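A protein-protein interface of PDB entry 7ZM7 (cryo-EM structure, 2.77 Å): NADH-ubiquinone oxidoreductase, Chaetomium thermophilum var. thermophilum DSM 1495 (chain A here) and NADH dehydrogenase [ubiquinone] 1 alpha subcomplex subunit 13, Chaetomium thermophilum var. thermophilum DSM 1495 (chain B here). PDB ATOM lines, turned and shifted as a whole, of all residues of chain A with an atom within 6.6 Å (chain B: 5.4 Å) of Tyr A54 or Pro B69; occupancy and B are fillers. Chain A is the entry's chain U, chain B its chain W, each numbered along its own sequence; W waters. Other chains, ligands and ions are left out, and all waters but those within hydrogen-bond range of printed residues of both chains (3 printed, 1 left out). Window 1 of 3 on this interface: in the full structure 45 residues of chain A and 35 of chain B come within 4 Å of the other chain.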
ATOM      1  N   ASP A  49      23.974 -14.485 -24.972  1.00  0.00           N
ATOM      2  CA  ASP A  49      24.671 -13.602 -24.008  1.00  0.00           C
ATOM      3  C   ASP A  49      24.831 -14.300 -22.676  1.00  0.00           C
ATOM      4  O   ASP A  49      25.924 -14.236 -22.123  1.00  0.00           O
ATOM      5  CB  ASP A  49      23.844 -12.350 -23.759  1.00  0.00           C
ATOM      6  CG  ASP A  49      23.992 -11.323 -24.871  1.00  0.00           C
ATOM      7  OD1 ASP A  49      24.697 -11.625 -25.854  1.00  0.00           O
ATOM      8  OD2 ASP A  49      23.407 -10.230 -24.743  1.00  0.00           O
ATOM      9  N   TYR A  50      23.794 -15.007 -22.252  1.00  0.00           N
ATOM     10  CA  TYR A  50      23.771 -15.719 -20.960  1.00  0.00           C
ATOM     11  C   TYR A  50      24.661 -16.947 -21.111  1.00  0.00           C
ATOM     12  O   TYR A  50      25.429 -17.239 -20.211  1.00  0.00           O
ATOM     13  CB  TYR A  50      22.311 -16.003 -20.649  1.00  0.00           C
ATOM     14  CG  TYR A  50      21.458 -14.777 -20.448  1.00  0.00           C
ATOM     15  CD1 TYR A  50      21.391 -14.153 -19.216  1.00  0.00           C
ATOM     16  CD2 TYR A  50      20.708 -14.252 -21.483  1.00  0.00           C
ATOM     17  CE1 TYR A  50      20.607 -13.030 -19.019  1.00  0.00           C
ATOM     18  CE2 TYR A  50      19.923 -13.127 -21.304  1.00  0.00           C
ATOM     19  CZ  TYR A  50      19.873 -12.513 -20.068  1.00  0.00           C
ATOM     20  OH  TYR A  50      19.101 -11.405 -19.885  1.00  0.00           O
ATOM     21  N   ASN A  51      24.575 -17.612 -22.258  1.00  0.00           N
ATOM     22  CA  ASN A  51      25.375 -18.828 -22.550  1.00  0.00           C
ATOM     23  C   ASN A  51      26.853 -18.461 -22.587  1.00  0.00           C
ATOM     24  O   ASN A  51      27.663 -19.283 -22.167  1.00  0.00           O
ATOM     25  CB  ASN A  51      24.923 -19.527 -23.838  1.00  0.00           C
ATOM     26  CG  ASN A  51      23.579 -20.213 -23.775  1.00  0.00           C
ATOM     27  OD1 ASN A  51      22.930 -20.231 -22.737  1.00  0.00           O
ATOM     28  ND2 ASN A  51      23.160 -20.783 -24.890  1.00  0.00           N
ATOM     29  N   ASP A  52      27.176 -17.274 -23.078  1.00  0.00           N
ATOM     30  CA  ASP A  52      28.590 -16.863 -23.240  1.00  0.00           C
ATOM     31  C   ASP A  52      29.091 -16.300 -21.922  1.00  0.00           C
ATOM     32  O   ASP A  52      30.256 -16.535 -21.595  1.00  0.00           O
ATOM     33  CB  ASP A  52      28.698 -15.870 -24.396  1.00  0.00           C
ATOM     34  CG  ASP A  52      28.930 -16.537 -25.737  1.00  0.00           C
ATOM     35  OD1 ASP A  52      29.814 -17.409 -25.807  1.00  0.00           O
ATOM     36  OD2 ASP A  52      28.222 -16.182 -26.696  1.00  0.00           O
ATOM     37  N   ASP A  53      28.209 -15.661 -21.151  1.00  0.00           N
ATOM     38  CA  ASP A  53      28.583 -15.128 -19.821  1.00  0.00           C
ATOM     39  C   ASP A  53      28.913 -16.298 -18.899  1.00  0.00           C
ATOM     40  O   ASP A  53      29.896 -16.201 -18.152  1.00  0.00           O
ATOM     41  CB  ASP A  53      27.452 -14.294 -19.233  1.00  0.00           C
ATOM     42  CG  ASP A  53      27.835 -13.527 -17.986  1.00  0.00           C
ATOM     43  OD1 ASP A  53      28.903 -12.899 -17.996  1.00  0.00           O
ATOM     44  OD2 ASP A  53      27.055 -13.569 -17.019  1.00  0.00           O
ATOM     45  N   TYR A  54      28.115 -17.358 -18.952  1.00  0.00           N
ATOM     46  CA  TYR A  54      28.324 -18.528 -18.064  1.00  0.00           C
ATOM     47  C   TYR A  54      29.668 -19.162 -18.372  1.00  0.00           C
ATOM     48  O   TYR A  54      30.353 -19.596 -17.445  1.00  0.00           O
ATOM     49  CB  TYR A  54      27.205 -19.551 -18.229  1.00  0.00           C
ATOM     50  CG  TYR A  54      27.441 -20.870 -17.541  1.00  0.00           C
ATOM     51  CD1 TYR A  54      27.433 -20.965 -16.161  1.00  0.00           C
ATOM     52  CD2 TYR A  54      27.676 -22.019 -18.272  1.00  0.00           C
ATOM     53  CE1 TYR A  54      27.653 -22.171 -15.522  1.00  0.00           C
ATOM     54  CE2 TYR A  54      27.895 -23.235 -17.650  1.00  0.00           C
ATOM     55  CZ  TYR A  54      27.885 -23.309 -16.271  1.00  0.00           C
ATOM     56  OH  TYR A  54      28.098 -24.504 -15.654  1.00  0.00           O
ATOM     57  N   MET A  55      30.048 -19.166 -19.637  1.00  0.00           N
ATOM     58  CA  MET A  55      31.283 -19.870 -20.041  1.00  0.00           C
ATOM     59  C   MET A  55      32.443 -18.946 -19.741  1.00  0.00           C
ATOM     60  O   MET A  55      33.527 -19.442 -19.454  1.00  0.00           O
ATOM     61  CB  MET A  55      31.227 -20.197 -21.537  1.00  0.00           C
ATOM     62  CG  MET A  55      30.171 -21.223 -21.868  1.00  0.00           C
ATOM     63  SD  MET A  55      30.478 -22.807 -21.069  1.00  0.00           S
ATOM     64  CE  MET A  55      31.878 -23.384 -22.024  1.00  0.00           C
ATOM     65  N   GLN A  56      32.172 -17.645 -19.717  1.00  0.00           N
ATOM     66  CA  GLN A  56      33.219 -16.693 -19.365  1.00  0.00           C
ATOM     67  C   GLN A  56      33.503 -16.678 -17.868  1.00  0.00           C
ATOM     68  O   GLN A  56      34.662 -16.621 -17.456  1.00  0.00           O
ATOM     69  CB  GLN A  56      32.810 -15.313 -19.843  1.00  0.00           C
ATOM     70  CG  GLN A  56      33.371 -14.938 -21.162  1.00  0.00           C
ATOM     71  CD  GLN A  56      33.104 -13.504 -21.479  1.00  0.00           C
ATOM     72  OE1 GLN A  56      31.997 -13.023 -21.293  1.00  0.00           O
ATOM     73  NE2 GLN A  56      34.115 -12.806 -21.962  1.00  0.00           N
ATOM     74  N   CYS A  57      32.456 -16.653 -17.046  1.00  0.00           N
ATOM     75  CA  CYS A  57      32.628 -16.735 -15.568  1.00  0.00           C
ATOM     76  C   CYS A  57      33.495 -17.945 -15.241  1.00  0.00           C
ATOM     77  O   CYS A  57      34.366 -17.818 -14.378  1.00  0.00           O
ATOM     78  CB  CYS A  57      31.286 -16.922 -14.866  1.00  0.00           C
ATOM     79  SG  CYS A  57      31.368 -17.192 -13.073  1.00  0.00           S
ATOM     80  N   LYS A  58      33.226 -19.090 -15.861  1.00  0.00           N
ATOM     81  CA  LYS A  58      33.981 -20.330 -15.541  1.00  0.00           C
ATOM     82  C   LYS A  58      35.436 -20.165 -15.968  1.00  0.00           C
ATOM     83  O   LYS A  58      36.313 -20.588 -15.214  1.00  0.00           O
ATOM     84  CB  LYS A  58      33.353 -21.516 -16.271  1.00  0.00           C
ATOM     85  CG  LYS A  58      31.978 -21.947 -15.788  1.00  0.00           C
ATOM     86  CD  LYS A  58      31.454 -23.136 -16.552  1.00  0.00           C
ATOM     87  CE  LYS A  58      32.301 -24.378 -16.375  1.00  0.00           C
ATOM     88  NZ  LYS A  58      32.362 -24.801 -14.958  1.00  0.00           N
ATOM     89  N   ASN A  59      35.663 -19.591 -17.145  1.00  0.00           N
ATOM     90  CA  ASN A  59      37.030 -19.336 -17.648  1.00  0.00           C
ATOM     91  C   ASN A  59      37.717 -18.343 -16.718  1.00  0.00           C
ATOM     92  O   ASN A  59      38.927 -18.491 -16.500  1.00  0.00           O
ATOM     93  CB  ASN A  59      37.003 -18.778 -19.068  1.00  0.00           C
ATOM     94  CG  ASN A  59      37.529 -19.744 -20.104  1.00  0.00           C
ATOM     95  OD1 ASN A  59      37.549 -20.949 -19.881  1.00  0.00           O
ATOM     96  ND2 ASN A  59      37.959 -19.223 -21.239  1.00  0.00           N
ATOM     97  N   GLY A  65      35.322 -23.217 -10.893  1.00  0.00           N
ATOM     98  CA  GLY A  65      34.167 -22.683 -11.633  1.00  0.00           C
ATOM     99  C   GLY A  65      32.885 -23.458 -11.527  1.00  0.00           C
ATOM    100  O   GLY A  65      31.879 -22.909 -11.980  1.00  0.00           O
ATOM    101  N   GLU A  66      32.888 -24.683 -11.004  1.00  0.00           N
ATOM    102  CA  GLU A  66      31.577 -25.344 -10.814  1.00  0.00           C
ATOM    103  C   GLU A  66      30.924 -24.548  -9.688  1.00  0.00           C
ATOM    104  O   GLU A  66      29.768 -24.166  -9.839  1.00  0.00           O
ATOM    105  CB  GLU A  66      31.822 -26.825 -10.508  1.00  0.00           C
ATOM    106  CG  GLU A  66      32.329 -27.623 -11.694  1.00  0.00           C
ATOM    107  CD  GLU A  66      33.732 -27.311 -12.189  1.00  0.00           C
ATOM    108  OE1 GLU A  66      34.565 -26.848 -11.377  1.00  0.00           O
ATOM    109  OE2 GLU A  66      33.988 -27.519 -13.392  1.00  0.00           O
ATOM    110  N   CYS A  69      30.244 -20.003 -10.015  1.00  0.00           N
ATOM    111  CA  CYS A  69      29.547 -19.634 -11.276  1.00  0.00           C
ATOM    112  C   CYS A  69      28.127 -20.199 -11.216  1.00  0.00           C
ATOM    113  O   CYS A  69      27.530 -20.345 -12.271  1.00  0.00           O
ATOM    114  CB  CYS A  69      30.323 -20.057 -12.519  1.00  0.00           C
ATOM    115  SG  CYS A  69      31.874 -19.149 -12.738  1.00  0.00           S
ATOM    116  N   LEU A  70      27.582 -20.453 -10.021  1.00  0.00           N
ATOM    117  CA  LEU A  70      26.244 -21.119  -9.914  1.00  0.00           C
ATOM    118  C   LEU A  70      25.084 -20.205 -10.327  1.00  0.00           C
ATOM    119  O   LEU A  70      24.166 -20.716 -10.973  1.00  0.00           O
ATOM    120  CB  LEU A  70      26.033 -21.750  -8.536  1.00  0.00           C
ATOM    121  CG  LEU A  70      26.824 -23.028  -8.267  1.00  0.00           C
ATOM    122  CD1 LEU A  70      26.650 -23.482  -6.830  1.00  0.00           C
ATOM    123  CD2 LEU A  70      26.414 -24.133  -9.224  1.00  0.00           C
ATOM    124  N   LYS A  71      25.155 -18.907 -10.030  1.00  0.00           N
ATOM    125  CA  LYS A  71      24.077 -17.969 -10.418  1.00  0.00           C
ATOM    126  C   LYS A  71      23.952 -17.891 -11.943  1.00  0.00           C
ATOM    127  O   LYS A  71      22.824 -17.837 -12.439  1.00  0.00           O
ATOM    128  CB  LYS A  71      24.311 -16.600  -9.786  1.00  0.00           C
ATOM    129  CG  LYS A  71      23.251 -15.547 -10.075  1.00  0.00           C
ATOM    130  CD  LYS A  71      23.442 -14.281  -9.273  1.00  0.00           C
ATOM    131  CE  LYS A  71      22.307 -13.294  -9.450  1.00  0.00           C
ATOM    132  NZ  LYS A  71      20.995 -13.902  -9.127  1.00  0.00           N
ATOM    133  N   GLU A  72      25.067 -17.877 -12.659  1.00  0.00           N
ATOM    134  CA  GLU A  72      25.077 -17.775 -14.134  1.00  0.00           C
ATOM    135  C   GLU A  72      24.423 -18.999 -14.767  1.00  0.00           C
ATOM    136  O   GLU A  72      23.701 -18.825 -15.746  1.00  0.00           O
ATOM    137  CB  GLU A  72      26.514 -17.558 -14.594  1.00  0.00           C
ATOM    138  CG  GLU A  72      27.072 -16.186 -14.258  1.00  0.00           C
ATOM    139  CD  GLU A  72      27.733 -16.045 -12.897  1.00  0.00           C
ATOM    140  OE1 GLU A  72      27.663 -17.000 -12.100  1.00  0.00           O
ATOM    141  OE2 GLU A  72      28.327 -14.981 -12.640  1.00  0.00           O
ATOM    142  N   GLY A  73      24.691 -20.192 -14.250  1.00  0.00           N
ATOM    143  CA  GLY A  73      24.072 -21.425 -14.780  1.00  0.00           C
ATOM    144  C   GLY A  73      22.577 -21.401 -14.613  1.00  0.00           C
ATOM    145  O   GLY A  73      21.880 -21.859 -15.531  1.00  0.00           O
ATOM    146  N   ARG A  74      22.101 -20.876 -13.481  1.00  0.00           N
ATOM    147  CA  ARG A  74      20.639 -20.761 -13.268  1.00  0.00           C
ATOM    148  C   ARG A  74      20.078 -19.776 -14.300  1.00  0.00           C
ATOM    149  O   ARG A  74      18.960 -20.008 -14.782  1.00  0.00           O
ATOM    150  CB  ARG A  74      20.344 -20.371 -11.820  1.00  0.00           C
ATOM    151  CG  ARG A  74      20.877 -21.359 -10.795  1.00  0.00           C
ATOM    152  CD  ARG A  74      20.323 -21.103  -9.409  1.00  0.00           C
ATOM    153  NE  ARG A  74      20.613 -19.780  -8.877  1.00  0.00           N
ATOM    154  CZ  ARG A  74      21.649 -19.486  -8.101  1.00  0.00           C
ATOM    155  NH1 ARG A  74      22.515 -20.425  -7.763  1.00  0.00           N
ATOM    156  NH2 ARG A  74      21.817 -18.252  -7.664  1.00  0.00           N
ATOM    157  N   VAL A  76      21.181 -19.317 -17.417  1.00  0.00           N
ATOM    158  CA  VAL A  76      21.100 -20.047 -18.722  1.00  0.00           C
ATOM    159  C   VAL A  76      19.899 -21.003 -18.766  1.00  0.00           C
ATOM    160  O   VAL A  76      19.232 -21.035 -19.795  1.00  0.00           O
ATOM    161  CB  VAL A  76      22.424 -20.718 -19.159  1.00  0.00           C
ATOM    162  CG1 VAL A  76      23.626 -19.827 -18.920  1.00  0.00           C
ATOM    163  CG2 VAL A  76      22.646 -22.096 -18.568  1.00  0.00           C
ATOM    164  N   THR A  77      19.585 -21.688 -17.661  1.00  0.00           N
ATOM    165  CA  THR A  77      18.517 -22.720 -17.683  1.00  0.00           C
ATOM    166  C   THR A  77      17.151 -22.033 -17.627  1.00  0.00           C
ATOM    167  O   THR A  77      16.144 -22.720 -17.845  1.00  0.00           O
ATOM    168  CB  THR A  77      18.721 -23.769 -16.585  1.00  0.00           C
ATOM    169  OG1 THR A  77      17.743 -24.795 -16.750  1.00  0.00           O
ATOM    170  CG2 THR A  77      18.593 -23.195 -15.195  1.00  0.00           C
ATOM    171  N   ILE B  65      27.160 -26.376 -29.564  1.00  0.00           N
ATOM    172  CA  ILE B  65      27.460 -25.122 -28.809  1.00  0.00           C
ATOM    173  C   ILE B  65      26.280 -24.434 -28.128  1.00  0.00           C
ATOM    174  O   ILE B  65      26.411 -24.131 -26.942  1.00  0.00           O
ATOM    175  CB  ILE B  65      28.294 -24.169 -29.686  1.00  0.00           C
ATOM    176  CG1 ILE B  65      29.695 -24.730 -29.936  1.00  0.00           C
ATOM    177  CG2 ILE B  65      28.324 -22.762 -29.107  1.00  0.00           C
ATOM    178  CD1 ILE B  65      30.314 -24.285 -31.237  1.00  0.00           C
ATOM    179  N   HIS B  66      25.150 -24.228 -28.800  1.00  0.00           N
ATOM    180  CA  HIS B  66      24.049 -23.474 -28.142  1.00  0.00           C
ATOM    181  C   HIS B  66      23.459 -24.297 -26.991  1.00  0.00           C
ATOM    182  O   HIS B  66      22.763 -23.703 -26.157  1.00  0.00           O
ATOM    183  CB  HIS B  66      23.007 -23.008 -29.161  1.00  0.00           C
ATOM    184  CG  HIS B  66      23.559 -22.165 -30.258  1.00  0.00           C
ATOM    185  ND1 HIS B  66      24.515 -21.195 -30.037  1.00  0.00           N
ATOM    186  CD2 HIS B  66      23.276 -22.122 -31.577  1.00  0.00           C
ATOM    187  CE1 HIS B  66      24.809 -20.601 -31.174  1.00  0.00           C
ATOM    188  NE2 HIS B  66      24.063 -21.153 -32.135  1.00  0.00           N
ATOM    189  N   LEU B  67      23.718 -25.607 -26.952  1.00  0.00           N
ATOM    190  CA  LEU B  67      23.261 -26.477 -25.845  1.00  0.00           C
ATOM    191  C   LEU B  67      24.340 -26.740 -24.797  1.00  0.00           C
ATOM    192  O   LEU B  67      23.966 -27.152 -23.714  1.00  0.00           O
ATOM    193  CB  LEU B  67      22.844 -27.797 -26.478  1.00  0.00           C
ATOM    194  CG  LEU B  67      21.733 -27.728 -27.512  1.00  0.00           C
ATOM    195  CD1 LEU B  67      21.658 -29.051 -28.251  1.00  0.00           C
ATOM    196  CD2 LEU B  67      20.410 -27.377 -26.856  1.00  0.00           C
ATOM    197  N   ILE B  68      25.618 -26.501 -25.082  1.00  0.00           N
ATOM    198  CA  ILE B  68      26.709 -26.892 -24.134  1.00  0.00           C
ATOM    199  C   ILE B  68      26.554 -26.181 -22.784  1.00  0.00           C
ATOM    200  O   ILE B  68      26.696 -26.875 -21.781  1.00  0.00           O
ATOM    201  CB  ILE B  68      28.114 -26.717 -24.750  1.00  0.00           C
ATOM    202  CG1 ILE B  68      28.586 -27.968 -25.489  1.00  0.00           C
ATOM    203  CG2 ILE B  68      29.139 -26.283 -23.713  1.00  0.00           C
ATOM    204  CD1 ILE B  68      29.853 -27.761 -26.275  1.00  0.00           C
ATOM    205  N   PRO B  69      26.252 -24.864 -22.686  1.00  0.00           N
ATOM    206  CA  PRO B  69      26.045 -24.219 -21.385  1.00  0.00           C
ATOM    207  C   PRO B  69      24.862 -24.719 -20.540  1.00  0.00           C
ATOM    208  O   PRO B  69      25.081 -24.862 -19.391  1.00  0.00           O
ATOM    209  CB  PRO B  69      26.026 -22.717 -21.725  1.00  0.00           C
ATOM    210  CG  PRO B  69      26.698 -22.634 -23.063  1.00  0.00           C
ATOM    211  CD  PRO B  69      26.211 -23.875 -23.767  1.00  0.00           C
ATOM    212  N   LEU B  70      23.682 -24.969 -21.104  1.00  0.00           N
ATOM    213  CA  LEU B  70      22.565 -25.593 -20.328  1.00  0.00           C
ATOM    214  C   LEU B  70      22.988 -26.973 -19.823  1.00  0.00           C
ATOM    215  O   LEU B  70      22.757 -27.255 -18.645  1.00  0.00           O
ATOM    216  CB  LEU B  70      21.225 -25.613 -21.079  1.00  0.00           C
ATOM    217  CG  LEU B  70      21.042 -26.562 -22.262  1.00  0.00           C
ATOM    218  CD1 LEU B  70      20.348 -27.850 -21.834  1.00  0.00           C
ATOM    219  CD2 LEU B  70      20.211 -25.883 -23.333  1.00  0.00           C
ATOM    220  N   LEU B  71      23.538 -27.816 -20.675  1.00  0.00           N
ATOM    221  CA  LEU B  71      23.861 -29.196 -20.246  1.00  0.00           C
ATOM    222  C   LEU B  71      24.941 -29.176 -19.171  1.00  0.00           C
ATOM    223  O   LEU B  71      24.855 -30.003 -18.258  1.00  0.00           O
ATOM    224  CB  LEU B  71      24.233 -30.053 -21.460  1.00  0.00           C
ATOM    225  CG  LEU B  71      23.082 -30.391 -22.402  1.00  0.00           C
ATOM    226  CD1 LEU B  71      23.602 -30.726 -23.786  1.00  0.00           C
ATOM    227  CD2 LEU B  71      22.250 -31.530 -21.845  1.00  0.00           C
ATOM    228  N   GLN B  72      25.937 -28.307 -19.312  1.00  0.00           N
ATOM    229  CA  GLN B  72      27.045 -28.172 -18.344  1.00  0.00           C
ATOM    230  C   GLN B  72      26.518 -27.633 -17.020  1.00  0.00           C
ATOM    231  O   GLN B  72      26.982 -28.094 -15.982  1.00  0.00           O
ATOM    232  CB  GLN B  72      28.127 -27.290 -18.962  1.00  0.00           C
ATOM    233  CG  GLN B  72      29.425 -27.263 -18.173  1.00  0.00           C
ATOM    234  CD  GLN B  72      30.063 -28.626 -18.098  1.00  0.00           C
ATOM    235  OE1 GLN B  72      30.045 -29.402 -19.049  1.00  0.00           O
ATOM    236  NE2 GLN B  72      30.649 -28.925 -16.952  1.00  0.00           N
ATOM    237  N   ALA B  73      25.583 -26.701 -17.075  1.00  0.00           N
ATOM    238  CA  ALA B  73      25.041 -26.057 -15.864  1.00  0.00           C
ATOM    239  C   ALA B  73      24.335 -27.094 -15.005  1.00  0.00           C
ATOM    240  O   ALA B  73      24.487 -27.038 -13.777  1.00  0.00           O
ATOM    241  CB  ALA B  73      24.131 -24.932 -16.280  1.00  0.00           C
ATOM    242  N   GLU B  74      23.597 -28.000 -15.637  1.00  0.00           N
ATOM    243  CA  GLU B  74      22.912 -29.078 -14.901  1.00  0.00           C
ATOM    244  C   GLU B  74      23.952 -29.984 -14.244  1.00  0.00           C
ATOM    245  O   GLU B  74      23.748 -30.344 -13.079  1.00  0.00           O
ATOM    246  CB  GLU B  74      22.047 -29.839 -15.892  1.00  0.00           C
ATOM    247  CG  GLU B  74      21.111 -30.819 -15.225  1.00  0.00           C
ATOM    248  CD  GLU B  74      20.815 -32.054 -16.050  1.00  0.00           C
ATOM    249  OE1 GLU B  74      20.772 -31.944 -17.290  1.00  0.00           O
ATOM    250  OE2 GLU B  74      20.647 -33.121 -15.445  1.00  0.00           O
ATOM    251  N   ASP B  76      27.036 -29.211 -13.401  1.00  0.00           N
ATOM    252  CA  ASP B  76      27.761 -28.434 -12.371  1.00  0.00           C
ATOM    253  C   ASP B  76      26.968 -28.401 -11.062  1.00  0.00           C
ATOM    254  O   ASP B  76      27.590 -28.530 -10.006  1.00  0.00           O
ATOM    255  CB  ASP B  76      28.134 -27.064 -12.929  1.00  0.00           C
ATOM    256  CG  ASP B  76      29.268 -27.139 -13.931  1.00  0.00           C
ATOM    257  OD1 ASP B  76      29.690 -28.265 -14.239  1.00  0.00           O
ATOM    258  OD2 ASP B  76      29.727 -26.075 -14.384  1.00  0.00           O
HETATM  259  O   HOH W   1      19.857 -27.000 -17.054  1.00  0.00           O
HETATM  260  O   HOH W   2      22.855 -23.882 -23.514  1.00  0.00           O
HETATM  261  O   HOH W   3      33.599 -28.122 -16.788  1.00  0.00           O
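O of His B66 lies within hydrogen-bond range of ND2 of Asn A51.
The side-chain carboxylate (OD2) of Asp B76 lies within hydrogen-bond range of the side-chain hydroxyl (OH) of Tyr A54 (2.6 Å).
The side-chain carboxylate (OD2) of Asp B76 lies within salt-bridge range of the side-chain amino group (NZ) of Lys A58 (3.0 Å).
The side-chain amino group (NZ) of Lys A58 is in salt-bridge range of the side-chain carboxylate (OE2) of Glu A66.
The side-chain sulfur of Cys A69 is in hydrogen-bond range of the backbone NH of Lys A58 (3.4 Å).
The side-chain amide nitrogen (NE2) of Gln B72 sits at hydrogen-bond distance from the side-chain carboxylate (OD1) of Asp B76 (3.0 Å).
SG of Cys A57 forms a disulfide with SG of Cys A69, at 2.0 Å.
Asn A51 touches Pro B69 (O to CG, 3.6 Å).
Pro B69 touches Tyr A54.
Gln B72 touches Tyr A54 (C to OH, 3.8 Å).
Ala B73 touches Tyr A54.
Pro B69 touches Met A55.
OD1 of Asp B76 touches CG of Glu A66 (3.7 Å).
Ala B73 touches Gly A73.
CG2 of Val A76 touches O of Pro B69 (3.8 Å).
CG2 of Val A76 touches CA of Leu B70, at 3.9 Å.
Val A76 touches Ala B73 (CG2 to CB, 3.9 Å).
Tyr A54 touches just these residues of chain B: Pro B69 (3.7 Å), Gln B72 (3.8 Å), Ala B73 (3.4 Å) and Asp B76 (2.6 Å).
Of chain A, only Asn A51 (3.6 Å), Tyr A54 (3.7 Å), Met A55 (3.9 Å) and Val A76 (3.8 Å) come within 4 Å of Pro B69.
Printed residues of chain A within 4 Å of Gln B72: Tyr A54.
Printed residues of chain B within 4 Å of Glu A66: Asp B76.
Leu B67 touches none of the printed residues of chain A.
Of the 21 printed residues of chain A, 7 touch a printed residue of chain B.
Along chain A the printed residues that touch a printed residue of chain B span positions 51 to 76.
Among the printed residues, Asp or Glu carboxylates within 4 Å of a Lys or Arg side-chain nitrogen of the other chain: Lys A58 with Asp B76 (3.0 Å).
Water W2 lies within hydrogen-bond range of the backbone carbonyl oxygen of His B66 (2.7 Å), the backbone NH of Leu B70 (2.8 Å), the side-chain amide nitrogen of Asn A51 (3.4 Å) and the backbone carbonyl oxygen of Leu B67 (3.5 Å).
Water W3 lies within hydrogen-bond range of the side-chain amide nitrogen (NE2) of Gln B72 (3.1 Å) and the side-chain carboxylate (OE2) of Glu A66 (3.5 Å).
Water W1 lies within hydrogen-bond range of OG1 of Thr A77 (3.1 Å) and O of Leu B70 (3.3 Å).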
